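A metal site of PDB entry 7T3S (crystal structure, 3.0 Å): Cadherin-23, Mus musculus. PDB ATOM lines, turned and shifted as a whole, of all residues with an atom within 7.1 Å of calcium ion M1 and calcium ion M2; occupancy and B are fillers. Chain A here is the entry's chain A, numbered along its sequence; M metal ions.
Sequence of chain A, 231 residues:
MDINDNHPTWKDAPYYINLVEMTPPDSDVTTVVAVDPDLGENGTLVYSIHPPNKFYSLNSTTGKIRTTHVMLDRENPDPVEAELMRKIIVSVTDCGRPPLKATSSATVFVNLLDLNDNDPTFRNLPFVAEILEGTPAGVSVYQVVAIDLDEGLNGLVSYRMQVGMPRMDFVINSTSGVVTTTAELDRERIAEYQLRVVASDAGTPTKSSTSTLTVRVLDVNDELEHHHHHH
The side-chain carboxylate of Glu 21 is in hydrogen-bond range of the backbone NH of Arg 74 (2.8 Å). The side-chain carboxylate (OE2) of Glu 75 lies within salt-bridge range of the guanidinium group (NE) of Arg 74, at 2.7 Å. The side-chain amino group (NZ) of Lys 207 lies within hydrogen-bond range of the backbone carbonyl oxygen (O) of Asp 117. N of Lys 207 is in hydrogen-bond range of OD1 of Asp 201. The backbone NH of Glu 75 is in hydrogen-bond range of the side-chain carboxylate of Asp 73, 3.2 Å away. The side-chain carboxylate of Asp 114 sits at hydrogen-bond distance from the backbone NH of Glu 151. The backbone NH of Glu 21 sits at hydrogen-bond distance from the backbone carbonyl oxygen of Leu 113 (3.0 Å). The backbone NH (N) of Gly 203 sits at hydrogen-bond distance from the side-chain carboxylate (OD1) of Asp 201.
Calcium ion M2 is bound by OD1 of Asn 116 (2.1 Å). Calcium ion M2 is bound by O of Asn 118, 2.3 Å away. Calcium ion M2 is bound by the side-chain carboxylate (OD2) of Asp 201 (2.4 Å). OD2 of Asp 148 is bound to calcium ion M2, at 2.4 Å. Calcium ion M2 is bound by OD2 of Asp 150 (2.4 Å). Calcium ion M2 is bound by O of Asn 154, 2.5 Å away. Calcium ion M2 is bound by OD1 of Asp 148. Calcium ion M2 has seven donor atoms within binding distance.
Within 4 Å of calcium ion M2: Asn 116, Asn 118, Asp 148, Asp 150, Asn 154 and Asp 201. The nearest printed residue that does not touch calcium ion M2 is Asp 119 (4.3 Å).
Calcium ion M1 is bound by O of Leu 115, OE2 of Glu 21, OD1 of Asp 114, OD1 of Asp 117, OE1 of Glu 75 and OD1 of Asp 150. Slightly farther from calcium ion M1 lies OE2 of Glu 75 (3.0 Å).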
ATOM      1  N   GLU A  21      -1.599  -9.837 -21.307  1.00  0.00           N
ATOM      2  CA  GLU A  21      -1.203 -11.178 -21.804  1.00  0.00           C
ATOM      3  C   GLU A  21       0.041 -11.618 -21.041  1.00  0.00           C
ATOM      4  O   GLU A  21       0.723 -10.749 -20.501  1.00  0.00           O
ATOM      5  CB  GLU A  21      -0.955 -11.149 -23.322  1.00  0.00           C
ATOM      6  CG  GLU A  21       0.311 -10.426 -23.743  1.00  0.00           C
ATOM      7  CD  GLU A  21       0.599 -10.498 -25.214  1.00  0.00           C
ATOM      8  OE1 GLU A  21       0.458 -11.627 -25.800  1.00  0.00           O
ATOM      9  OE2 GLU A  21       0.977  -9.440 -25.808  1.00  0.00           O
ATOM     10  N   MET A  22       0.288 -12.933 -20.997  1.00  0.00           N
ATOM     11  CA  MET A  22       1.428 -13.579 -20.280  1.00  0.00           C
ATOM     12  C   MET A  22       1.277 -13.396 -18.751  1.00  0.00           C
ATOM     13  O   MET A  22       2.186 -13.834 -18.008  1.00  0.00           O
ATOM     14  CB  MET A  22       2.799 -13.027 -20.747  1.00  0.00           C
ATOM     15  CG  MET A  22       3.076 -13.239 -22.236  1.00  0.00           C
ATOM     16  SD  MET A  22       3.152 -15.009 -22.688  1.00  0.00           S
ATOM     17  CE  MET A  22       3.165 -14.930 -24.475  1.00  0.00           C
ATOM     18  N   ASP A  73      -1.698 -15.593 -24.721  1.00  0.00           N
ATOM     19  CA  ASP A  73      -0.888 -15.070 -25.847  1.00  0.00           C
ATOM     20  C   ASP A  73      -1.824 -14.325 -26.800  1.00  0.00           C
ATOM     21  O   ASP A  73      -2.677 -14.993 -27.413  1.00  0.00           O
ATOM     22  CB  ASP A  73      -0.131 -16.232 -26.503  1.00  0.00           C
ATOM     23  CG  ASP A  73       0.871 -15.832 -27.573  1.00  0.00           C
ATOM     24  OD1 ASP A  73       0.948 -14.613 -27.901  1.00  0.00           O
ATOM     25  OD2 ASP A  73       1.571 -16.733 -28.055  1.00  0.00           O
ATOM     26  N   ARG A  74      -1.686 -12.986 -26.932  1.00  0.00           N
ATOM     27  CA  ARG A  74      -2.584 -12.124 -27.785  1.00  0.00           C
ATOM     28  C   ARG A  74      -2.377 -12.475 -29.269  1.00  0.00           C
ATOM     29  O   ARG A  74      -3.333 -12.339 -30.028  1.00  0.00           O
ATOM     30  CB  ARG A  74      -2.316 -10.628 -27.553  1.00  0.00           C
ATOM     31  CG  ARG A  74      -3.484  -9.724 -27.964  1.00  0.00           C
ATOM     32  CD  ARG A  74      -3.077  -8.271 -28.213  1.00  0.00           C
ATOM     33  NE  ARG A  74      -2.169  -8.175 -29.343  1.00  0.00           N
ATOM     34  CZ  ARG A  74      -2.512  -8.284 -30.651  1.00  0.00           C
ATOM     35  NH1 ARG A  74      -1.577  -8.191 -31.592  1.00  0.00           N
ATOM     36  NH2 ARG A  74      -3.781  -8.484 -31.019  1.00  0.00           N
ATOM     37  N   GLU A  75      -1.174 -12.921 -29.621  1.00  0.00           N
ATOM     38  CA  GLU A  75      -0.764 -13.285 -31.003  1.00  0.00           C
ATOM     39  C   GLU A  75      -0.947 -14.804 -31.261  1.00  0.00           C
ATOM     40  O   GLU A  75      -0.423 -15.276 -32.299  1.00  0.00           O
ATOM     41  CB  GLU A  75       0.681 -12.827 -31.242  1.00  0.00           C
ATOM     42  CG  GLU A  75       0.850 -11.301 -31.290  1.00  0.00           C
ATOM     43  CD  GLU A  75       0.768 -10.549 -29.967  1.00  0.00           C
ATOM     44  OE1 GLU A  75       1.366 -11.024 -28.989  1.00  0.00           O
ATOM     45  OE2 GLU A  75       0.137  -9.497 -29.926  1.00  0.00           O
ATOM     46  N   LEU A 113      -4.757  -7.285 -23.170  1.00  0.00           N
ATOM     47  CA  LEU A 113      -3.875  -6.130 -23.405  1.00  0.00           C
ATOM     48  C   LEU A 113      -2.524  -6.664 -23.882  1.00  0.00           C
ATOM     49  O   LEU A 113      -2.108  -7.734 -23.416  1.00  0.00           O
ATOM     50  CB  LEU A 113      -3.766  -5.298 -22.131  1.00  0.00           C
ATOM     51  CG  LEU A 113      -5.073  -4.630 -21.712  1.00  0.00           C
ATOM     52  CD1 LEU A 113      -4.956  -4.030 -20.320  1.00  0.00           C
ATOM     53  CD2 LEU A 113      -5.491  -3.577 -22.741  1.00  0.00           C
ATOM     54  N   ASP A 114      -1.902  -5.917 -24.795  1.00  0.00           N
ATOM     55  CA  ASP A 114      -0.716  -6.319 -25.574  1.00  0.00           C
ATOM     56  C   ASP A 114       0.553  -5.941 -24.832  1.00  0.00           C
ATOM     57  O   ASP A 114       0.603  -4.876 -24.275  1.00  0.00           O
ATOM     58  CB  ASP A 114      -0.703  -5.628 -26.939  1.00  0.00           C
ATOM     59  CG  ASP A 114       0.445  -6.067 -27.826  1.00  0.00           C
ATOM     60  OD1 ASP A 114       0.596  -7.300 -28.042  1.00  0.00           O
ATOM     61  OD2 ASP A 114       1.173  -5.191 -28.292  1.00  0.00           O
ATOM     62  N   LEU A 115       1.522  -6.829 -24.851  1.00  0.00           N
ATOM     63  CA  LEU A 115       2.916  -6.571 -24.458  1.00  0.00           C
ATOM     64  C   LEU A 115       3.743  -6.608 -25.718  1.00  0.00           C
ATOM     65  O   LEU A 115       3.326  -7.297 -26.653  1.00  0.00           O
ATOM     66  CB  LEU A 115       3.404  -7.644 -23.474  1.00  0.00           C
ATOM     67  CG  LEU A 115       2.787  -7.633 -22.085  1.00  0.00           C
ATOM     68  CD1 LEU A 115       3.454  -8.700 -21.218  1.00  0.00           C
ATOM     69  CD2 LEU A 115       2.891  -6.259 -21.436  1.00  0.00           C
ATOM     70  N   ASN A 116       4.869  -5.922 -25.719  1.00  0.00           N
ATOM     71  CA  ASN A 116       5.873  -5.992 -26.802  1.00  0.00           C
ATOM     72  C   ASN A 116       6.678  -7.275 -26.569  1.00  0.00           C
ATOM     73  O   ASN A 116       7.867  -7.172 -26.339  1.00  0.00           O
ATOM     74  CB  ASN A 116       6.732  -4.721 -26.858  1.00  0.00           C
ATOM     75  CG  ASN A 116       7.463  -4.554 -28.173  1.00  0.00           C
ATOM     76  OD1 ASN A 116       7.197  -5.244 -29.150  1.00  0.00           O
ATOM     77  ND2 ASN A 116       8.406  -3.634 -28.212  1.00  0.00           N
ATOM     78  N   ASP A 117       6.022  -8.419 -26.636  1.00  0.00           N
ATOM     79  CA  ASP A 117       6.622  -9.729 -26.282  1.00  0.00           C
ATOM     80  C   ASP A 117       7.182 -10.408 -27.549  1.00  0.00           C
ATOM     81  O   ASP A 117       8.020 -11.341 -27.393  1.00  0.00           O
ATOM     82  CB  ASP A 117       5.615 -10.599 -25.508  1.00  0.00           C
ATOM     83  CG  ASP A 117       4.435 -11.087 -26.317  1.00  0.00           C
ATOM     84  OD1 ASP A 117       4.033 -10.378 -27.284  1.00  0.00           O
ATOM     85  OD2 ASP A 117       3.896 -12.186 -25.979  1.00  0.00           O
ATOM     86  N   ASN A 118       6.739  -9.975 -28.755  1.00  0.00           N
ATOM     87  CA  ASN A 118       7.239 -10.464 -30.061  1.00  0.00           C
ATOM     88  C   ASN A 118       8.215  -9.450 -30.670  1.00  0.00           C
ATOM     89  O   ASN A 118       8.036  -8.231 -30.457  1.00  0.00           O
ATOM     90  CB  ASN A 118       6.103 -10.751 -31.037  1.00  0.00           C
ATOM     91  CG  ASN A 118       5.284 -11.951 -30.652  1.00  0.00           C
ATOM     92  OD1 ASN A 118       5.271 -12.358 -29.486  1.00  0.00           O
ATOM     93  ND2 ASN A 118       4.590 -12.529 -31.610  1.00  0.00           N
ATOM     94  N   ASP A 119       9.215  -9.960 -31.400  1.00  0.00           N
ATOM     95  CA  ASP A 119      10.239  -9.196 -32.153  1.00  0.00           C
ATOM     96  C   ASP A 119       9.887  -9.240 -33.639  1.00  0.00           C
ATOM     97  O   ASP A 119       9.067 -10.069 -34.061  1.00  0.00           O
ATOM     98  CB  ASP A 119      11.664  -9.728 -31.877  1.00  0.00           C
ATOM     99  CG  ASP A 119      11.809 -11.246 -31.936  1.00  0.00           C
ATOM    100  OD1 ASP A 119      11.152 -11.889 -32.812  1.00  0.00           O
ATOM    101  OD2 ASP A 119      12.570 -11.798 -31.106  1.00  0.00           O
ATOM    102  N   PRO A 120      10.463  -8.352 -34.498  1.00  0.00           N
ATOM    103  CA  PRO A 120      10.220  -8.429 -35.927  1.00  0.00           C
ATOM    104  C   PRO A 120      10.804  -9.733 -36.499  1.00  0.00           C
ATOM    105  O   PRO A 120      11.839 -10.190 -35.994  1.00  0.00           O
ATOM    106  CB  PRO A 120      10.939  -7.178 -36.499  1.00  0.00           C
ATOM    107  CG  PRO A 120      11.147  -6.271 -35.290  1.00  0.00           C
ATOM    108  CD  PRO A 120      11.350  -7.223 -34.142  1.00  0.00           C
ATOM    109  N   ASP A 148       5.797  -7.759 -37.573  1.00  0.00           N
ATOM    110  CA  ASP A 148       5.766  -7.904 -36.103  1.00  0.00           C
ATOM    111  C   ASP A 148       4.294  -8.115 -35.715  1.00  0.00           C
ATOM    112  O   ASP A 148       3.463  -7.207 -36.015  1.00  0.00           O
ATOM    113  CB  ASP A 148       6.441  -6.711 -35.448  1.00  0.00           C
ATOM    114  CG  ASP A 148       6.600  -6.806 -33.940  1.00  0.00           C
ATOM    115  OD1 ASP A 148       5.719  -7.385 -33.274  1.00  0.00           O
ATOM    116  OD2 ASP A 148       7.609  -6.296 -33.437  1.00  0.00           O
ATOM    117  N   LEU A 149       3.994  -9.250 -35.066  1.00  0.00           N
ATOM    118  CA  LEU A 149       2.608  -9.716 -34.785  1.00  0.00           C
ATOM    119  C   LEU A 149       1.966  -8.902 -33.659  1.00  0.00           C
ATOM    120  O   LEU A 149       0.747  -8.995 -33.493  1.00  0.00           O
ATOM    121  CB  LEU A 149       2.641 -11.207 -34.415  1.00  0.00           C
ATOM    122  CG  LEU A 149       3.175 -12.154 -35.502  1.00  0.00           C
ATOM    123  CD1 LEU A 149       3.255 -13.585 -34.991  1.00  0.00           C
ATOM    124  CD2 LEU A 149       2.317 -12.077 -36.773  1.00  0.00           C
ATOM    125  N   ASP A 150       2.762  -8.132 -32.911  1.00  0.00           N
ATOM    126  CA  ASP A 150       2.271  -7.240 -31.836  1.00  0.00           C
ATOM    127  C   ASP A 150       1.340  -6.164 -32.426  1.00  0.00           C
ATOM    128  O   ASP A 150       1.271  -6.036 -33.675  1.00  0.00           O
ATOM    129  CB  ASP A 150       3.418  -6.615 -31.040  1.00  0.00           C
ATOM    130  CG  ASP A 150       4.198  -7.598 -30.190  1.00  0.00           C
ATOM    131  OD1 ASP A 150       3.636  -8.645 -29.793  1.00  0.00           O
ATOM    132  OD2 ASP A 150       5.347  -7.301 -29.929  1.00  0.00           O
ATOM    133  N   GLU A 151       0.664  -5.435 -31.530  1.00  0.00           N
ATOM    134  CA  GLU A 151      -0.419  -4.455 -31.811  1.00  0.00           C
ATOM    135  C   GLU A 151       0.143  -3.034 -31.816  1.00  0.00           C
ATOM    136  O   GLU A 151       1.117  -2.775 -31.082  1.00  0.00           O
ATOM    137  CB  GLU A 151      -1.495  -4.618 -30.728  1.00  0.00           C
ATOM    138  CG  GLU A 151      -2.780  -3.859 -30.964  1.00  0.00           C
ATOM    139  CD  GLU A 151      -3.866  -4.191 -29.940  1.00  0.00           C
ATOM    140  OE1 GLU A 151      -4.110  -5.410 -29.697  1.00  0.00           O
ATOM    141  OE2 GLU A 151      -4.474  -3.240 -29.386  1.00  0.00           O
ATOM    142  N   LEU A 153       1.923   0.410 -32.141  1.00  0.00           N
ATOM    143  CA  LEU A 153       3.346   0.825 -32.241  1.00  0.00           C
ATOM    144  C   LEU A 153       4.265  -0.389 -32.040  1.00  0.00           C
ATOM    145  O   LEU A 153       5.293  -0.436 -32.691  1.00  0.00           O
ATOM    146  CB  LEU A 153       3.640   1.919 -31.212  1.00  0.00           C
ATOM    147  CG  LEU A 153       2.914   3.264 -31.442  1.00  0.00           C
ATOM    148  CD1 LEU A 153       3.115   4.183 -30.261  1.00  0.00           C
ATOM    149  CD2 LEU A 153       3.387   3.937 -32.733  1.00  0.00           C
ATOM    150  N   ASN A 154       3.880  -1.349 -31.190  1.00  0.00           N
ATOM    151  CA  ASN A 154       4.693  -2.566 -30.868  1.00  0.00           C
ATOM    152  C   ASN A 154       4.879  -3.454 -32.116  1.00  0.00           C
ATOM    153  O   ASN A 154       5.810  -4.249 -32.103  1.00  0.00           O
ATOM    154  CB  ASN A 154       4.088  -3.398 -29.741  1.00  0.00           C
ATOM    155  CG  ASN A 154       4.137  -2.704 -28.392  1.00  0.00           C
ATOM    156  OD1 ASN A 154       5.155  -2.133 -28.020  1.00  0.00           O
ATOM    157  ND2 ASN A 154       3.050  -2.764 -27.667  1.00  0.00           N
ATOM    158  N   GLY A 155       4.017  -3.337 -33.130  1.00  0.00           N
ATOM    159  CA  GLY A 155       4.067  -4.125 -34.376  1.00  0.00           C
ATOM    160  C   GLY A 155       4.600  -3.331 -35.556  1.00  0.00           C
ATOM    161  O   GLY A 155       4.726  -3.937 -36.624  1.00  0.00           O
ATOM    162  N   LEU A 156       4.909  -2.050 -35.375  1.00  0.00           N
ATOM    163  CA  LEU A 156       5.321  -1.139 -36.484  1.00  0.00           C
ATOM    164  C   LEU A 156       6.833  -1.283 -36.727  1.00  0.00           C
ATOM    165  O   LEU A 156       7.624  -0.725 -35.924  1.00  0.00           O
ATOM    166  CB  LEU A 156       4.916   0.295 -36.124  1.00  0.00           C
ATOM    167  CG  LEU A 156       5.422   1.393 -37.071  1.00  0.00           C
ATOM    168  CD1 LEU A 156       5.117   1.076 -38.522  1.00  0.00           C
ATOM    169  CD2 LEU A 156       4.842   2.743 -36.686  1.00  0.00           C
ATOM    170  N   ASP A 201      11.019  -2.404 -33.962  1.00  0.00           N
ATOM    171  CA  ASP A 201       9.602  -1.990 -33.780  1.00  0.00           C
ATOM    172  C   ASP A 201       9.618  -0.667 -33.032  1.00  0.00           C
ATOM    173  O   ASP A 201      10.708  -0.150 -32.825  1.00  0.00           O
ATOM    174  CB  ASP A 201       8.791  -3.090 -33.099  1.00  0.00           C
ATOM    175  CG  ASP A 201       9.287  -3.520 -31.736  1.00  0.00           C
ATOM    176  OD1 ASP A 201      10.026  -2.747 -31.095  1.00  0.00           O
ATOM    177  OD2 ASP A 201       8.925  -4.616 -31.315  1.00  0.00           O
ATOM    178  N   ALA A 202       8.443  -0.142 -32.642  1.00  0.00           N
ATOM    179  CA  ALA A 202       8.297   1.189 -32.001  1.00  0.00           C
ATOM    180  C   ALA A 202       7.902   1.069 -30.504  1.00  0.00           C
ATOM    181  O   ALA A 202       7.327   2.042 -29.969  1.00  0.00           O
ATOM    182  CB  ALA A 202       7.294   2.012 -32.782  1.00  0.00           C
ATOM    183  N   GLY A 203       8.194  -0.061 -29.834  1.00  0.00           N
ATOM    184  CA  GLY A 203       7.965  -0.215 -28.388  1.00  0.00           C
ATOM    185  C   GLY A 203       8.976   0.597 -27.591  1.00  0.00           C
ATOM    186  O   GLY A 203      10.084   0.820 -28.109  1.00  0.00           O
ATOM    187  N   PRO A 205      10.594  -0.314 -24.842  1.00  0.00           N
ATOM    188  CA  PRO A 205      11.771  -1.177 -24.811  1.00  0.00           C
ATOM    189  C   PRO A 205      11.838  -1.858 -26.205  1.00  0.00           C
ATOM    190  O   PRO A 205      11.311  -2.950 -26.368  1.00  0.00           O
ATOM    191  CB  PRO A 205      11.425  -2.124 -23.661  1.00  0.00           C
ATOM    192  CG  PRO A 205       9.856  -2.215 -23.698  1.00  0.00           C
ATOM    193  CD  PRO A 205       9.375  -1.097 -24.627  1.00  0.00           C
ATOM    194  N   LYS A 207      12.456  -3.801 -29.602  1.00  0.00           N
ATOM    195  CA  LYS A 207      12.884  -5.186 -29.937  1.00  0.00           C
ATOM    196  C   LYS A 207      13.339  -5.212 -31.397  1.00  0.00           C
ATOM    197  O   LYS A 207      12.607  -4.668 -32.259  1.00  0.00           O
ATOM    198  CB  LYS A 207      11.760  -6.180 -29.687  1.00  0.00           C
ATOM    199  CG  LYS A 207      11.335  -6.292 -28.243  1.00  0.00           C
ATOM    200  CD  LYS A 207      10.680  -7.592 -27.885  1.00  0.00           C
ATOM    201  CE  LYS A 207      11.653  -8.761 -27.892  1.00  0.00           C
ATOM    202  NZ  LYS A 207      10.989 -10.021 -27.463  1.00  0.00           N
HETATM  203 CA    CA M   1       2.180  -8.985 -27.720  1.00  0.00          CA
HETATM  204 CA    CA M   2       7.155  -6.148 -31.095  1.00  0.00          CA
